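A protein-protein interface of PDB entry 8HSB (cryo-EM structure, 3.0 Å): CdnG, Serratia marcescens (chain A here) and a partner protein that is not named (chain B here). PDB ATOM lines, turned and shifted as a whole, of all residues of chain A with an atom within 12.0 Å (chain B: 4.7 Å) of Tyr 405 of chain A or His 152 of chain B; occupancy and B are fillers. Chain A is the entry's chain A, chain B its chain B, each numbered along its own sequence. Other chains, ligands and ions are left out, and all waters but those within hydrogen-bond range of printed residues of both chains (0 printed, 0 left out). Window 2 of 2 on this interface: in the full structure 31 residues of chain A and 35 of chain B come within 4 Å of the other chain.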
ATOM      1  N   ARG A 371      22.563  12.427  -5.506  1.00  0.00           N
ATOM      2  CA  ARG A 371      21.236  11.925  -5.160  1.00  0.00           C
ATOM      3  C   ARG A 371      21.168  11.542  -3.689  1.00  0.00           C
ATOM      4  O   ARG A 371      20.237  11.935  -2.976  1.00  0.00           O
ATOM      5  CB  ARG A 371      20.860  10.717  -6.017  1.00  0.00           C
ATOM      6  CG  ARG A 371      19.476  10.178  -5.659  1.00  0.00           C
ATOM      7  CD  ARG A 371      19.082   8.916  -6.413  1.00  0.00           C
ATOM      8  NE  ARG A 371      18.834   9.127  -7.833  1.00  0.00           N
ATOM      9  CZ  ARG A 371      18.581   8.149  -8.693  1.00  0.00           C
ATOM     10  NH1 ARG A 371      18.529   6.885  -8.306  1.00  0.00           N
ATOM     11  NH2 ARG A 371      18.368   8.447  -9.969  1.00  0.00           N
ATOM     12  N   LYS A 401      13.700  11.157  -2.780  1.00  0.00           N
ATOM     13  CA  LYS A 401      13.980   9.770  -3.129  1.00  0.00           C
ATOM     14  C   LYS A 401      12.955   9.257  -4.134  1.00  0.00           C
ATOM     15  O   LYS A 401      11.749   9.465  -3.979  1.00  0.00           O
ATOM     16  CB  LYS A 401      13.983   8.902  -1.868  1.00  0.00           C
ATOM     17  CG  LYS A 401      14.428   7.463  -2.087  1.00  0.00           C
ATOM     18  CD  LYS A 401      13.245   6.512  -2.106  1.00  0.00           C
ATOM     19  CE  LYS A 401      12.656   6.345  -0.716  1.00  0.00           C
ATOM     20  NZ  LYS A 401      11.503   5.405  -0.716  1.00  0.00           N
ATOM     21  N   ASN A 402      13.446   8.578  -5.170  1.00  0.00           N
ATOM     22  CA  ASN A 402      12.604   8.148  -6.276  1.00  0.00           C
ATOM     23  C   ASN A 402      13.092   6.806  -6.804  1.00  0.00           C
ATOM     24  O   ASN A 402      14.260   6.446  -6.640  1.00  0.00           O
ATOM     25  CB  ASN A 402      12.593   9.190  -7.399  1.00  0.00           C
ATOM     26  CG  ASN A 402      13.990   9.606  -7.821  1.00  0.00           C
ATOM     27  OD1 ASN A 402      14.985   9.138  -7.267  1.00  0.00           O
ATOM     28  ND2 ASN A 402      14.070  10.495  -8.799  1.00  0.00           N
ATOM     29  N   THR A 403      12.180   6.069  -7.437  1.00  0.00           N
ATOM     30  CA  THR A 403      12.481   4.778  -8.046  1.00  0.00           C
ATOM     31  C   THR A 403      12.022   4.794  -9.498  1.00  0.00           C
ATOM     32  O   THR A 403      10.879   5.163  -9.786  1.00  0.00           O
ATOM     33  CB  THR A 403      11.805   3.632  -7.289  1.00  0.00           C
ATOM     34  OG1 THR A 403      10.395   3.657  -7.544  1.00  0.00           O
ATOM     35  CG2 THR A 403      12.052   3.754  -5.792  1.00  0.00           C
ATOM     36  N   PHE A 404      12.910   4.388 -10.404  1.00  0.00           N
ATOM     37  CA  PHE A 404      12.633   4.341 -11.837  1.00  0.00           C
ATOM     38  C   PHE A 404      12.682   2.895 -12.314  1.00  0.00           C
ATOM     39  O   PHE A 404      13.762   2.304 -12.409  1.00  0.00           O
ATOM     40  CB  PHE A 404      13.626   5.194 -12.624  1.00  0.00           C
ATOM     41  CG  PHE A 404      13.604   6.651 -12.266  1.00  0.00           C
ATOM     42  CD1 PHE A 404      12.487   7.219 -11.676  1.00  0.00           C
ATOM     43  CD2 PHE A 404      14.695   7.457 -12.537  1.00  0.00           C
ATOM     44  CE1 PHE A 404      12.464   8.558 -11.355  1.00  0.00           C
ATOM     45  CE2 PHE A 404      14.677   8.797 -12.219  1.00  0.00           C
ATOM     46  CZ  PHE A 404      13.559   9.348 -11.628  1.00  0.00           C
ATOM     47  N   TYR A 405      11.516   2.332 -12.614  1.00  0.00           N
ATOM     48  CA  TYR A 405      11.456   1.044 -13.283  1.00  0.00           C
ATOM     49  C   TYR A 405      11.857   1.201 -14.749  1.00  0.00           C
ATOM     50  O   TYR A 405      11.369   2.078 -15.468  1.00  0.00           O
ATOM     51  CB  TYR A 405      10.054   0.445 -13.168  1.00  0.00           C
ATOM     52  CG  TYR A 405       9.750  -0.632 -14.187  1.00  0.00           C
ATOM     53  CD1 TYR A 405      10.534  -1.776 -14.277  1.00  0.00           C
ATOM     54  CD2 TYR A 405       8.680  -0.503 -15.063  1.00  0.00           C
ATOM     55  CE1 TYR A 405      10.259  -2.761 -15.208  1.00  0.00           C
ATOM     56  CE2 TYR A 405       8.397  -1.484 -15.998  1.00  0.00           C
ATOM     57  CZ  TYR A 405       9.190  -2.609 -16.066  1.00  0.00           C
ATOM     58  OH  TYR A 405       8.913  -3.587 -16.994  1.00  0.00           O
ATOM     59  N   GLY A 406      12.763   0.334 -15.191  1.00  0.00           N
ATOM     60  CA  GLY A 406      13.282   0.399 -16.546  1.00  0.00           C
ATOM     61  C   GLY A 406      12.245   0.157 -17.626  1.00  0.00           C
ATOM     62  O   GLY A 406      11.124  -0.265 -17.343  1.00  0.00           O
ATOM     63  N   HIS B  87       9.870   2.620 -22.306  1.00  0.00           N
ATOM     64  CA  HIS B  87       8.433   2.690 -22.036  1.00  0.00           C
ATOM     65  C   HIS B  87       7.673   3.430 -23.133  1.00  0.00           C
ATOM     66  O   HIS B  87       6.924   4.371 -22.864  1.00  0.00           O
ATOM     67  CB  HIS B  87       8.153   3.329 -20.672  1.00  0.00           C
ATOM     68  CG  HIS B  87       8.521   2.463 -19.510  1.00  0.00           C
ATOM     69  ND1 HIS B  87       8.546   2.928 -18.213  1.00  0.00           N
ATOM     70  CD2 HIS B  87       8.877   1.157 -19.448  1.00  0.00           C
ATOM     71  CE1 HIS B  87       8.906   1.949 -17.403  1.00  0.00           C
ATOM     72  NE2 HIS B  87       9.112   0.863 -18.127  1.00  0.00           N
ATOM     73  N   TYR B  89       4.643   3.560 -24.709  1.00  0.00           N
ATOM     74  CA  TYR B  89       3.404   3.026 -24.169  1.00  0.00           C
ATOM     75  C   TYR B  89       2.220   3.732 -24.813  1.00  0.00           C
ATOM     76  O   TYR B  89       2.372   4.819 -25.380  1.00  0.00           O
ATOM     77  CB  TYR B  89       3.361   3.192 -22.643  1.00  0.00           C
ATOM     78  CG  TYR B  89       4.131   2.124 -21.894  1.00  0.00           C
ATOM     79  CD1 TYR B  89       4.470   0.926 -22.511  1.00  0.00           C
ATOM     80  CD2 TYR B  89       4.528   2.318 -20.577  1.00  0.00           C
ATOM     81  CE1 TYR B  89       5.176  -0.053 -21.834  1.00  0.00           C
ATOM     82  CE2 TYR B  89       5.234   1.345 -19.892  1.00  0.00           C
ATOM     83  CZ  TYR B  89       5.555   0.161 -20.526  1.00  0.00           C
ATOM     84  OH  TYR B  89       6.258  -0.812 -19.852  1.00  0.00           O
ATOM     85  N   CYS B 101       7.363   6.159 -16.004  1.00  0.00           N
ATOM     86  CA  CYS B 101       7.085   5.986 -14.585  1.00  0.00           C
ATOM     87  C   CYS B 101       8.081   6.805 -13.772  1.00  0.00           C
ATOM     88  O   CYS B 101       9.284   6.793 -14.057  1.00  0.00           O
ATOM     89  CB  CYS B 101       7.156   4.510 -14.206  1.00  0.00           C
ATOM     90  SG  CYS B 101       8.758   3.733 -14.517  1.00  0.00           S
ATOM     91  N   TRP B 133      15.234  10.917 -15.081  1.00  0.00           N
ATOM     92  CA  TRP B 133      14.944   9.715 -15.854  1.00  0.00           C
ATOM     93  C   TRP B 133      15.554   9.805 -17.246  1.00  0.00           C
ATOM     94  O   TRP B 133      16.141   8.836 -17.741  1.00  0.00           O
ATOM     95  CB  TRP B 133      13.429   9.504 -15.941  1.00  0.00           C
ATOM     96  CG  TRP B 133      13.024   8.108 -16.328  1.00  0.00           C
ATOM     97  CD1 TRP B 133      12.563   7.132 -15.495  1.00  0.00           C
ATOM     98  CD2 TRP B 133      13.037   7.537 -17.644  1.00  0.00           C
ATOM     99  NE1 TRP B 133      12.292   5.988 -16.207  1.00  0.00           N
ATOM    100  CE2 TRP B 133      12.574   6.211 -17.528  1.00  0.00           C
ATOM    101  CE3 TRP B 133      13.394   8.017 -18.908  1.00  0.00           C
ATOM    102  CZ2 TRP B 133      12.462   5.363 -18.626  1.00  0.00           C
ATOM    103  CZ3 TRP B 133      13.282   7.172 -19.993  1.00  0.00           C
ATOM    104  CH2 TRP B 133      12.822   5.860 -19.847  1.00  0.00           C
ATOM    105  N   GLY B 150      17.629   0.223 -10.042  1.00  0.00           N
ATOM    106  CA  GLY B 150      17.305  -1.025 -10.705  1.00  0.00           C
ATOM    107  C   GLY B 150      16.166  -1.790 -10.063  1.00  0.00           C
ATOM    108  O   GLY B 150      16.362  -2.909  -9.580  1.00  0.00           O
ATOM    109  N   LYS B 151      14.973  -1.203 -10.049  1.00  0.00           N
ATOM    110  CA  LYS B 151      13.801  -1.856  -9.483  1.00  0.00           C
ATOM    111  C   LYS B 151      12.896  -2.343 -10.608  1.00  0.00           C
ATOM    112  O   LYS B 151      12.432  -1.546 -11.429  1.00  0.00           O
ATOM    113  CB  LYS B 151      13.047  -0.898  -8.558  1.00  0.00           C
ATOM    114  CG  LYS B 151      11.932  -1.545  -7.748  1.00  0.00           C
ATOM    115  CD  LYS B 151      10.566  -1.273  -8.353  1.00  0.00           C
ATOM    116  CE  LYS B 151       9.457  -1.851  -7.489  1.00  0.00           C
ATOM    117  NZ  LYS B 151       8.109  -1.570  -8.056  1.00  0.00           N
ATOM    118  N   HIS B 152      12.646  -3.652 -10.638  1.00  0.00           N
ATOM    119  CA  HIS B 152      11.845  -4.250 -11.698  1.00  0.00           C
ATOM    120  C   HIS B 152      11.294  -5.600 -11.254  1.00  0.00           C
ATOM    121  O   HIS B 152      12.057  -6.478 -10.833  1.00  0.00           O
ATOM    122  CB  HIS B 152      12.677  -4.406 -12.972  1.00  0.00           C
ATOM    123  CG  HIS B 152      13.915  -5.227 -12.789  1.00  0.00           C
ATOM    124  ND1 HIS B 152      15.051  -4.735 -12.182  1.00  0.00           N
ATOM    125  CD2 HIS B 152      14.196  -6.506 -13.131  1.00  0.00           C
ATOM    126  CE1 HIS B 152      15.977  -5.676 -12.158  1.00  0.00           C
ATOM    127  NE2 HIS B 152      15.485  -6.761 -12.728  1.00  0.00           N
ATOM    128  N   PRO B 153       9.978  -5.801 -11.321  1.00  0.00           N
ATOM    129  CA  PRO B 153       9.408  -7.094 -10.926  1.00  0.00           C
ATOM    130  C   PRO B 153       9.214  -8.042 -12.101  1.00  0.00           C
ATOM    131  O   PRO B 153       9.184  -7.615 -13.259  1.00  0.00           O
ATOM    132  CB  PRO B 153       8.063  -6.702 -10.296  1.00  0.00           C
ATOM    133  CG  PRO B 153       7.842  -5.225 -10.656  1.00  0.00           C
ATOM    134  CD  PRO B 153       8.927  -4.815 -11.606  1.00  0.00           C
ATOM    135  N   ARG B 154       9.086  -9.333 -11.806  1.00  0.00           N
ATOM    136  CA  ARG B 154       8.778 -10.334 -12.815  1.00  0.00           C
ATOM    137  C   ARG B 154       7.268 -10.537 -12.910  1.00  0.00           C
ATOM    138  O   ARG B 154       6.541 -10.279 -11.948  1.00  0.00           O
ATOM    139  CB  ARG B 154       9.479 -11.647 -12.478  1.00  0.00           C
ATOM    140  CG  ARG B 154      10.950 -11.667 -12.861  1.00  0.00           C
ATOM    141  CD  ARG B 154      11.507 -13.082 -12.871  1.00  0.00           C
ATOM    142  NE  ARG B 154      12.838 -13.148 -12.280  1.00  0.00           N
ATOM    143  CZ  ARG B 154      13.592 -14.238 -12.254  1.00  0.00           C
ATOM    144  NH1 ARG B 154      13.175 -15.380 -12.778  1.00  0.00           N
ATOM    145  NH2 ARG B 154      14.795 -14.182 -11.689  1.00  0.00           N
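Among the printed residues, merely in contact across the chains: Phe 404 of chain A with Trp 133 of chain B (3.4 Å), Tyr 405 of chain A with His 87 of chain B (3.1 Å), Tyr 405 of chain A with Lys 151 of chain B (3.3 Å) and Tyr 405 of chain A with His 152 of chain B (3.6 Å).
Printed residues of chain B within 4 Å of Tyr 405 of chain A: His 87, Cys 101, Lys 151 and His 152.
Printed residues of chain B within 4 Å of Gly 406 of chain A: His 87.
Of the printed residues of chain A, Trp 133 of chain B touches Phe 404.
No residue of chain A comes within 4 Å of Gly 150 of chain B.
Of chain A, only Tyr 405 (3.3 Å) comes within 4 Å of Lys 151 of chain B.
His 152 of chain B touches just one residue of chain A: Tyr 405 (3.6 Å).
No residue of chain A comes within 4 Å of Pro 153 of chain B.
The nearest residue of chain B that does not touch Tyr 405 of chain A is Trp 133 of chain B (4.1 Å).
The nearest printed residue of chain B that does not touch Phe 404 of chain A is Cys 101 of chain B (4.01 Å).
Of the 7 printed residues of chain A, 3 touch a printed residue of chain B.
Printed residues of chain B that touch a printed residue of chain A: His 87, Cys 101, Trp 133, Lys 151 and His 152.
Hydrophobic or aromatic side chains of chain B that line the printed part of chain A: His 87, Trp 133 and His 152.
Among the printed residues, 6 pairs touch across the chains.
SG of Cys 101 of chain B sits at hydrogen-bond distance from O of Tyr 405 of chain A, at 3.2 Å.
O of Gly 406 of chain A is in hydrogen-bond range of NE2 of His 87 of chain B, at 2.4 Å.
The backbone carbonyl oxygen of Gly 150 of chain B sits at hydrogen-bond distance from a ring nitrogen (ND1) of His 152 of chain B (3.4 Å).
A ring nitrogen (ND1) of His 87 of chain B sits close to the side-chain sulfur of Cys 101 of chain B, 3.8 Å away.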
